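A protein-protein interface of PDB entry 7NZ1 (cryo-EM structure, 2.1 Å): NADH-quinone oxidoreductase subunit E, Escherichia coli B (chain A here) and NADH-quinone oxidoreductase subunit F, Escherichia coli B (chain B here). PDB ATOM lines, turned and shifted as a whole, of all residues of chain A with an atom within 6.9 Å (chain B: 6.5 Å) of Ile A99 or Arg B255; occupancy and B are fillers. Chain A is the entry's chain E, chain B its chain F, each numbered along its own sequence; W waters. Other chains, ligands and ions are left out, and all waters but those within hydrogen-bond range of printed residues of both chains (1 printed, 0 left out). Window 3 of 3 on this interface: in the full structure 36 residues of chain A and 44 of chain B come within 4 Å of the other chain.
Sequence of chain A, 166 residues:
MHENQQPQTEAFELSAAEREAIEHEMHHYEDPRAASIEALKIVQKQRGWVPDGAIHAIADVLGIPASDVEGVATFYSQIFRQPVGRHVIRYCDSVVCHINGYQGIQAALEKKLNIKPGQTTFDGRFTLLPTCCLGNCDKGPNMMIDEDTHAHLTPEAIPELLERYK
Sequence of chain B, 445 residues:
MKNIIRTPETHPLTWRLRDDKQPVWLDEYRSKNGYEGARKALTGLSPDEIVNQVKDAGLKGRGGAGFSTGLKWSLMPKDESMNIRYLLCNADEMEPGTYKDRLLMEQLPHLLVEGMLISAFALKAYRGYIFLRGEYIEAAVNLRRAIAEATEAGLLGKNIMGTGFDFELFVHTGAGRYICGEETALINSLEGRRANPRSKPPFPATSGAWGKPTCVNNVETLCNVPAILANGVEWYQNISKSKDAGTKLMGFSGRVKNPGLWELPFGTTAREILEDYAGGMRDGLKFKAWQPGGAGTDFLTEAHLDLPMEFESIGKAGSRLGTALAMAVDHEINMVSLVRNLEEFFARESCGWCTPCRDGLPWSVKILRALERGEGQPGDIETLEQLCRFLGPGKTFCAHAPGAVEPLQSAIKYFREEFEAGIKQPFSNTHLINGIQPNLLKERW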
ATOM      1  N   SER A  94     -17.230  26.093  19.389  1.00  0.00           N
ATOM      2  CA  SER A  94     -17.665  26.537  18.075  1.00  0.00           C
ATOM      3  C   SER A  94     -17.381  25.434  17.058  1.00  0.00           C
ATOM      4  O   SER A  94     -17.054  24.306  17.421  1.00  0.00           O
ATOM      5  CB  SER A  94     -17.012  27.865  17.706  1.00  0.00           C
ATOM      6  OG  SER A  94     -17.203  28.814  18.730  1.00  0.00           O
ATOM      7  N   VAL A  95     -17.451  25.767  15.769  1.00  0.00           N
ATOM      8  CA  VAL A  95     -17.529  24.738  14.734  1.00  0.00           C
ATOM      9  C   VAL A  95     -16.170  24.082  14.447  1.00  0.00           C
ATOM     10  O   VAL A  95     -16.105  22.865  14.246  1.00  0.00           O
ATOM     11  CB  VAL A  95     -18.215  25.318  13.471  1.00  0.00           C
ATOM     12  CG1 VAL A  95     -17.416  26.421  12.777  1.00  0.00           C
ATOM     13  CG2 VAL A  95     -18.557  24.220  12.490  1.00  0.00           C
ATOM     14  N   VAL A  96     -15.072  24.844  14.433  1.00  0.00           N
ATOM     15  CA  VAL A  96     -13.777  24.236  14.127  1.00  0.00           C
ATOM     16  C   VAL A  96     -13.276  23.422  15.308  1.00  0.00           C
ATOM     17  O   VAL A  96     -12.640  22.373  15.131  1.00  0.00           O
ATOM     18  CB  VAL A  96     -12.768  25.320  13.713  1.00  0.00           C
ATOM     19  CG1 VAL A  96     -11.512  24.698  13.109  1.00  0.00           C
ATOM     20  CG2 VAL A  96     -13.406  26.281  12.747  1.00  0.00           C
ATOM     21  N   CYS A  97     -13.614  23.839  16.522  1.00  0.00           N
ATOM     22  CA  CYS A  97     -13.235  23.070  17.693  1.00  0.00           C
ATOM     23  C   CYS A  97     -14.126  21.842  17.849  1.00  0.00           C
ATOM     24  O   CYS A  97     -13.708  20.857  18.462  1.00  0.00           O
ATOM     25  CB  CYS A  97     -13.280  23.966  18.930  1.00  0.00           C
ATOM     26  SG  CYS A  97     -11.736  24.884  19.214  1.00  0.00           S
ATOM     27  N   HIS A  98     -15.349  21.893  17.309  1.00  0.00           N
ATOM     28  CA  HIS A  98     -16.215  20.716  17.271  1.00  0.00           C
ATOM     29  C   HIS A  98     -15.636  19.631  16.374  1.00  0.00           C
ATOM     30  O   HIS A  98     -15.757  18.443  16.687  1.00  0.00           O
ATOM     31  CB  HIS A  98     -17.629  21.147  16.840  1.00  0.00           C
ATOM     32  CG  HIS A  98     -18.541  20.031  16.422  1.00  0.00           C
ATOM     33  ND1 HIS A  98     -19.566  19.583  17.228  1.00  0.00           N
ATOM     34  CD2 HIS A  98     -18.677  19.371  15.246  1.00  0.00           C
ATOM     35  CE1 HIS A  98     -20.237  18.637  16.600  1.00  0.00           C
ATOM     36  NE2 HIS A  98     -19.716  18.486  15.396  1.00  0.00           N
ATOM     37  N   ILE A  99     -14.974  20.020  15.285  1.00  0.00           N
ATOM     38  CA  ILE A  99     -14.398  19.039  14.374  1.00  0.00           C
ATOM     39  C   ILE A  99     -13.129  18.434  14.976  1.00  0.00           C
ATOM     40  O   ILE A  99     -12.868  17.237  14.811  1.00  0.00           O
ATOM     41  CB  ILE A  99     -14.164  19.715  13.006  1.00  0.00           C
ATOM     42  CG1 ILE A  99     -15.499  19.940  12.299  1.00  0.00           C
ATOM     43  CG2 ILE A  99     -13.213  18.949  12.102  1.00  0.00           C
ATOM     44  CD1 ILE A  99     -15.456  21.013  11.279  1.00  0.00           C
ATOM     45  N   ASN A 100     -12.416  19.190  15.805  1.00  0.00           N
ATOM     46  CA  ASN A 100     -11.161  18.726  16.382  1.00  0.00           C
ATOM     47  C   ASN A 100     -11.335  18.035  17.728  1.00  0.00           C
ATOM     48  O   ASN A 100     -10.336  17.628  18.326  1.00  0.00           O
ATOM     49  CB  ASN A 100     -10.187  19.899  16.528  1.00  0.00           C
ATOM     50  CG  ASN A 100      -9.694  20.417  15.193  1.00  0.00           C
ATOM     51  OD1 ASN A 100      -9.296  19.643  14.328  1.00  0.00           O
ATOM     52  ND2 ASN A 100      -9.718  21.728  15.021  1.00  0.00           N
ATOM     53  N   GLY A 101     -12.565  17.872  18.212  1.00  0.00           N
ATOM     54  CA  GLY A 101     -12.789  17.020  19.364  1.00  0.00           C
ATOM     55  C   GLY A 101     -13.037  17.679  20.706  1.00  0.00           C
ATOM     56  O   GLY A 101     -12.540  17.175  21.718  1.00  0.00           O
ATOM     57  N   TYR A 102     -13.769  18.807  20.731  1.00  0.00           N
ATOM     58  CA  TYR A 102     -14.034  19.520  21.985  1.00  0.00           C
ATOM     59  C   TYR A 102     -14.860  18.676  22.953  1.00  0.00           C
ATOM     60  O   TYR A 102     -14.739  18.854  24.171  1.00  0.00           O
ATOM     61  CB  TYR A 102     -14.701  20.890  21.698  1.00  0.00           C
ATOM     62  CG  TYR A 102     -16.221  21.025  21.864  1.00  0.00           C
ATOM     63  CD1 TYR A 102     -16.817  21.273  23.111  1.00  0.00           C
ATOM     64  CD2 TYR A 102     -17.060  20.911  20.763  1.00  0.00           C
ATOM     65  CE1 TYR A 102     -18.179  21.359  23.246  1.00  0.00           C
ATOM     66  CE2 TYR A 102     -18.430  21.021  20.890  1.00  0.00           C
ATOM     67  CZ  TYR A 102     -18.983  21.248  22.134  1.00  0.00           C
ATOM     68  OH  TYR A 102     -20.347  21.355  22.275  1.00  0.00           O
ATOM     69  N   GLN A 103     -15.748  17.814  22.432  1.00  0.00           N
ATOM     70  CA  GLN A 103     -16.625  16.999  23.276  1.00  0.00           C
ATOM     71  C   GLN A 103     -15.840  16.044  24.170  1.00  0.00           C
ATOM     72  O   GLN A 103     -16.273  15.750  25.288  1.00  0.00           O
ATOM     73  CB  GLN A 103     -17.632  16.231  22.418  1.00  0.00           C
ATOM     74  CG  GLN A 103     -18.754  17.096  21.849  1.00  0.00           C
ATOM     75  CD  GLN A 103     -19.223  16.621  20.490  1.00  0.00           C
ATOM     76  OE1 GLN A 103     -19.187  17.371  19.515  1.00  0.00           O
ATOM     77  NE2 GLN A 103     -19.656  15.366  20.414  1.00  0.00           N
ATOM     78  N   SER B 253      -8.381  25.225   7.746  1.00  0.00           N
ATOM     79  CA  SER B 253      -8.418  24.690   9.095  1.00  0.00           C
ATOM     80  C   SER B 253      -9.316  23.464   9.119  1.00  0.00           C
ATOM     81  O   SER B 253     -10.148  23.262   8.233  1.00  0.00           O
ATOM     82  CB  SER B 253      -8.910  25.736  10.103  1.00  0.00           C
ATOM     83  OG  SER B 253     -10.265  26.067   9.868  1.00  0.00           O
ATOM     84  N   GLY B 254      -9.124  22.630  10.131  1.00  0.00           N
ATOM     85  CA  GLY B 254      -9.881  21.409  10.239  1.00  0.00           C
ATOM     86  C   GLY B 254      -8.949  20.243  10.421  1.00  0.00           C
ATOM     87  O   GLY B 254      -7.824  20.390  10.912  1.00  0.00           O
ATOM     88  N   ARG B 255      -9.431  19.057  10.061  1.00  0.00           N
ATOM     89  CA  ARG B 255      -8.604  17.852  10.112  1.00  0.00           C
ATOM     90  C   ARG B 255      -7.830  17.694   8.802  1.00  0.00           C
ATOM     91  O   ARG B 255      -8.061  16.795   7.992  1.00  0.00           O
ATOM     92  CB  ARG B 255      -9.460  16.641  10.448  1.00  0.00           C
ATOM     93  CG  ARG B 255     -10.182  16.817  11.768  1.00  0.00           C
ATOM     94  CD  ARG B 255     -10.414  15.515  12.502  1.00  0.00           C
ATOM     95  NE  ARG B 255     -11.628  14.822  12.094  1.00  0.00           N
ATOM     96  CZ  ARG B 255     -12.033  13.668  12.603  1.00  0.00           C
ATOM     97  NH1 ARG B 255     -11.334  13.042  13.538  1.00  0.00           N
ATOM     98  NH2 ARG B 255     -13.160  13.121  12.159  1.00  0.00           N
ATOM     99  N   VAL B 256      -6.887  18.615   8.613  1.00  0.00           N
ATOM    100  CA  VAL B 256      -5.987  18.650   7.472  1.00  0.00           C
ATOM    101  C   VAL B 256      -4.576  18.465   8.013  1.00  0.00           C
ATOM    102  O   VAL B 256      -4.338  18.560   9.222  1.00  0.00           O
ATOM    103  CB  VAL B 256      -6.092  19.957   6.657  1.00  0.00           C
ATOM    104  CG1 VAL B 256      -7.520  20.220   6.234  1.00  0.00           C
ATOM    105  CG2 VAL B 256      -5.532  21.123   7.441  1.00  0.00           C
ATOM    106  N   LYS B 257      -3.650  18.131   7.108  1.00  0.00           N
ATOM    107  CA  LYS B 257      -2.281  17.809   7.513  1.00  0.00           C
ATOM    108  C   LYS B 257      -1.556  19.018   8.095  1.00  0.00           C
ATOM    109  O   LYS B 257      -0.875  18.902   9.120  1.00  0.00           O
ATOM    110  CB  LYS B 257      -1.496  17.250   6.327  1.00  0.00           C
ATOM    111  CG  LYS B 257      -0.467  16.193   6.696  1.00  0.00           C
ATOM    112  CD  LYS B 257      -0.300  15.180   5.573  1.00  0.00           C
ATOM    113  CE  LYS B 257      -1.460  14.207   5.536  1.00  0.00           C
ATOM    114  NZ  LYS B 257      -1.525  13.458   4.254  1.00  0.00           N
ATOM    115  N   PRO B 259      -2.755  22.634   9.082  1.00  0.00           N
ATOM    116  CA  PRO B 259      -3.628  23.803   9.275  1.00  0.00           C
ATOM    117  C   PRO B 259      -2.807  25.053   9.561  1.00  0.00           C
ATOM    118  O   PRO B 259      -1.821  25.012  10.299  1.00  0.00           O
ATOM    119  CB  PRO B 259      -4.494  23.411  10.476  1.00  0.00           C
ATOM    120  CG  PRO B 259      -3.703  22.408  11.200  1.00  0.00           C
ATOM    121  CD  PRO B 259      -2.909  21.658  10.176  1.00  0.00           C
ATOM    122  N   GLY B 280      -3.400  18.608   2.336  1.00  0.00           N
ATOM    123  CA  GLY B 280      -4.499  17.671   2.192  1.00  0.00           C
ATOM    124  C   GLY B 280      -5.034  17.186   3.528  1.00  0.00           C
ATOM    125  O   GLY B 280      -4.607  17.600   4.603  1.00  0.00           O
ATOM    126  N   MET B 281      -5.996  16.274   3.438  1.00  0.00           N
ATOM    127  CA  MET B 281      -6.626  15.710   4.620  1.00  0.00           C
ATOM    128  C   MET B 281      -5.669  14.782   5.357  1.00  0.00           C
ATOM    129  O   MET B 281      -4.702  14.264   4.792  1.00  0.00           O
ATOM    130  CB  MET B 281      -7.891  14.951   4.237  1.00  0.00           C
ATOM    131  CG  MET B 281      -8.748  15.682   3.240  1.00  0.00           C
ATOM    132  SD  MET B 281      -9.401  17.200   3.946  1.00  0.00           S
ATOM    133  CE  MET B 281     -10.282  16.554   5.366  1.00  0.00           C
ATOM    134  N   ARG B 282      -5.939  14.597   6.647  1.00  0.00           N
ATOM    135  CA  ARG B 282      -5.184  13.641   7.439  1.00  0.00           C
ATOM    136  C   ARG B 282      -5.460  12.221   6.957  1.00  0.00           C
ATOM    137  O   ARG B 282      -6.485  11.935   6.332  1.00  0.00           O
ATOM    138  CB  ARG B 282      -5.536  13.761   8.919  1.00  0.00           C
ATOM    139  CG  ARG B 282      -4.745  14.811   9.670  1.00  0.00           C
ATOM    140  CD  ARG B 282      -4.878  14.598  11.167  1.00  0.00           C
ATOM    141  NE  ARG B 282      -5.762  15.566  11.805  1.00  0.00           N
ATOM    142  CZ  ARG B 282      -6.420  15.345  12.933  1.00  0.00           C
ATOM    143  NH1 ARG B 282      -6.332  14.188  13.569  1.00  0.00           N
ATOM    144  NH2 ARG B 282      -7.175  16.313  13.447  1.00  0.00           N
ATOM    145  N   LEU B 285      -8.809   9.909   6.212  1.00  0.00           N
ATOM    146  CA  LEU B 285      -9.969  10.780   6.114  1.00  0.00           C
ATOM    147  C   LEU B 285     -10.196  11.169   4.662  1.00  0.00           C
ATOM    148  O   LEU B 285      -9.242  11.423   3.920  1.00  0.00           O
ATOM    149  CB  LEU B 285      -9.799  12.036   6.972  1.00  0.00           C
ATOM    150  CG  LEU B 285      -9.493  11.839   8.453  1.00  0.00           C
ATOM    151  CD1 LEU B 285      -9.229  13.174   9.110  1.00  0.00           C
ATOM    152  CD2 LEU B 285     -10.630  11.105   9.149  1.00  0.00           C
ATOM    153  N   MET B 327     -12.648  26.114   6.034  1.00  0.00           N
ATOM    154  CA  MET B 327     -12.728  25.007   6.973  1.00  0.00           C
ATOM    155  C   MET B 327     -13.075  23.734   6.217  1.00  0.00           C
ATOM    156  O   MET B 327     -14.050  23.708   5.464  1.00  0.00           O
ATOM    157  CB  MET B 327     -13.767  25.295   8.058  1.00  0.00           C
ATOM    158  CG  MET B 327     -13.957  24.179   9.069  1.00  0.00           C
ATOM    159  SD  MET B 327     -15.376  24.492  10.132  1.00  0.00           S
ATOM    160  CE  MET B 327     -16.729  24.224   8.995  1.00  0.00           C
ATOM    161  N   ALA B 328     -12.295  22.680   6.430  1.00  0.00           N
ATOM    162  CA  ALA B 328     -12.529  21.398   5.776  1.00  0.00           C
ATOM    163  C   ALA B 328     -13.358  20.486   6.673  1.00  0.00           C
ATOM    164  O   ALA B 328     -13.091  20.378   7.873  1.00  0.00           O
ATOM    165  CB  ALA B 328     -11.205  20.724   5.421  1.00  0.00           C
ATOM    166  N   VAL B 329     -14.377  19.856   6.096  1.00  0.00           N
ATOM    167  CA  VAL B 329     -15.207  18.869   6.782  1.00  0.00           C
ATOM    168  C   VAL B 329     -14.920  17.508   6.167  1.00  0.00           C
ATOM    169  O   VAL B 329     -15.038  17.334   4.949  1.00  0.00           O
ATOM    170  CB  VAL B 329     -16.700  19.214   6.682  1.00  0.00           C
ATOM    171  CG1 VAL B 329     -17.533  18.211   7.457  1.00  0.00           C
ATOM    172  CG2 VAL B 329     -16.941  20.622   7.175  1.00  0.00           C
ATOM    173  N   ASP B 330     -14.535  16.545   6.999  1.00  0.00           N
ATOM    174  CA  ASP B 330     -14.226  15.223   6.488  1.00  0.00           C
ATOM    175  C   ASP B 330     -15.453  14.309   6.558  1.00  0.00           C
ATOM    176  O   ASP B 330     -16.537  14.712   6.983  1.00  0.00           O
ATOM    177  CB  ASP B 330     -12.984  14.668   7.203  1.00  0.00           C
ATOM    178  CG  ASP B 330     -13.129  14.554   8.724  1.00  0.00           C
ATOM    179  OD1 ASP B 330     -14.144  14.059   9.250  1.00  0.00           O
ATOM    180  OD2 ASP B 330     -12.188  14.988   9.418  1.00  0.00           O
ATOM    181  N   HIS B 331     -15.271  13.048   6.163  1.00  0.00           N
ATOM    182  CA  HIS B 331     -16.389  12.122   6.012  1.00  0.00           C
ATOM    183  C   HIS B 331     -16.943  11.601   7.334  1.00  0.00           C
ATOM    184  O   HIS B 331     -17.991  10.948   7.326  1.00  0.00           O
ATOM    185  CB  HIS B 331     -15.973  10.941   5.132  1.00  0.00           C
ATOM    186  CG  HIS B 331     -15.124   9.930   5.837  1.00  0.00           C
ATOM    187  ND1 HIS B 331     -13.777  10.114   6.055  1.00  0.00           N
ATOM    188  CD2 HIS B 331     -15.431   8.725   6.371  1.00  0.00           C
ATOM    189  CE1 HIS B 331     -13.289   9.064   6.692  1.00  0.00           C
ATOM    190  NE2 HIS B 331     -14.273   8.207   6.896  1.00  0.00           N
ATOM    191  N   GLU B 332     -16.284  11.864   8.459  1.00  0.00           N
ATOM    192  CA  GLU B 332     -16.716  11.348   9.751  1.00  0.00           C
ATOM    193  C   GLU B 332     -17.567  12.326  10.551  1.00  0.00           C
ATOM    194  O   GLU B 332     -18.048  11.961  11.626  1.00  0.00           O
ATOM    195  CB  GLU B 332     -15.507  10.927  10.584  1.00  0.00           C
ATOM    196  CG  GLU B 332     -14.487  10.134   9.812  1.00  0.00           C
ATOM    197  CD  GLU B 332     -13.610   9.296  10.710  1.00  0.00           C
ATOM    198  OE1 GLU B 332     -12.786   9.879  11.442  1.00  0.00           O
ATOM    199  OE2 GLU B 332     -13.747   8.056  10.683  1.00  0.00           O
ATOM    200  N   ILE B 333     -17.755  13.552  10.073  1.00  0.00           N
ATOM    201  CA  ILE B 333     -18.624  14.514  10.743  1.00  0.00           C
ATOM    202  C   ILE B 333     -20.033  14.380  10.180  1.00  0.00           C
ATOM    203  O   ILE B 333     -20.241  14.502   8.969  1.00  0.00           O
ATOM    204  CB  ILE B 333     -18.115  15.956  10.585  1.00  0.00           C
ATOM    205  CG1 ILE B 333     -16.830  16.191  11.373  1.00  0.00           C
ATOM    206  CG2 ILE B 333     -19.169  16.958  11.017  1.00  0.00           C
ATOM    207  CD1 ILE B 333     -15.689  16.603  10.516  1.00  0.00           C
ATOM    208  N   LEU B 338     -23.091  19.040  12.766  1.00  0.00           N
ATOM    209  CA  LEU B 338     -22.279  20.208  12.426  1.00  0.00           C
ATOM    210  C   LEU B 338     -23.123  21.471  12.294  1.00  0.00           C
ATOM    211  O   LEU B 338     -22.716  22.549  12.741  1.00  0.00           O
ATOM    212  CB  LEU B 338     -21.528  19.950  11.125  1.00  0.00           C
ATOM    213  CG  LEU B 338     -20.357  20.884  10.847  1.00  0.00           C
ATOM    214  CD1 LEU B 338     -19.219  20.609  11.813  1.00  0.00           C
ATOM    215  CD2 LEU B 338     -19.920  20.738   9.412  1.00  0.00           C
HETATM  216  O   HOH W   1      -7.916  23.346  12.777  1.00  0.00           O
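O of Val A96 sits at hydrogen-bond distance from ND2 of Asn A100, 3.0 Å away.
A ring nitrogen (ND1) of His A98 sits at hydrogen-bond distance from the side-chain amide oxygen of Gln A103 (3.2 Å).
The backbone NH (N) of Ala B328 sits at hydrogen-bond distance from the backbone carbonyl oxygen (O) of Ser B253.
The backbone carbonyl oxygen of Arg B255 lies within hydrogen-bond range of the backbone NH of Arg B282.
The side-chain carboxylate (OD2) of Asp B330 is in salt-bridge range of the guanidinium group (NE) of Arg B255, 2.7 Å away.
The guanidinium group (NH2) of Arg B255 is in salt-bridge range of the side-chain carboxylate (OE1) of Glu B332.
Water W1 lies within hydrogen-bond range of the backbone NH of Gly B254 (3.0 Å) and the side-chain amide nitrogen of Asn A100 (3.3 Å).
Ile A99 touches just these residues of chain B: Arg B255, Met B327, Ile B333 and Leu B338.
Printed residues of chain B within 4 Å of Asn A100: Gly B254 and Arg B255.
Of the printed residues of chain A, Ser B253 touches Val A96 (3.7 Å).
Of the printed residues of chain A, Gly B254 touches Asn A100 (3.8 Å).
Of chain A, only Ile A99 (3.7 Å) and Asn A100 (3.9 Å) come within 4 Å of Arg B255.
Met B281 touches none of the printed residues of chain A.
The nearest residue of chain B that does not touch Ile A99 is Ala B328 (4.2 Å).
Along chain B the printed residues that touch a printed residue of chain A span positions 253 to 338.
Of the 10 printed residues of chain A, 5 touch a printed residue of chain B.
Hydrophobic or aromatic side chains of chain A that line the printed part of chain B: Val A95, Val A96, His A98 and Ile A99.
Among the printed residues, 11 pairs touch across the chains.
Among the printed residues, no Asp or Glu carboxylate lies within 4 Å of a Lys or Arg side-chain nitrogen of the other chain.
Among the printed residues, merely in contact across the chains: Ile A99 with Met B327 (3.7 Å), His A98 with Leu B338 (3.7 Å), Ile A99 with Arg B255 (3.7 Å), Val A96 with Met B327 (3.7 Å), Val A96 with Ser B253 (3.7 Å), Val A95 with Leu B338 (3.7 Å), Ile A99 with Ile B333 (3.8 Å), Asn A100 with Gly B254 (3.8 Å), Ile A99 with Leu B338 (3.8 Å), Val A95 with Met B327 (3.9 Å) and Asn A100 with Arg B255 (3.9 Å).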
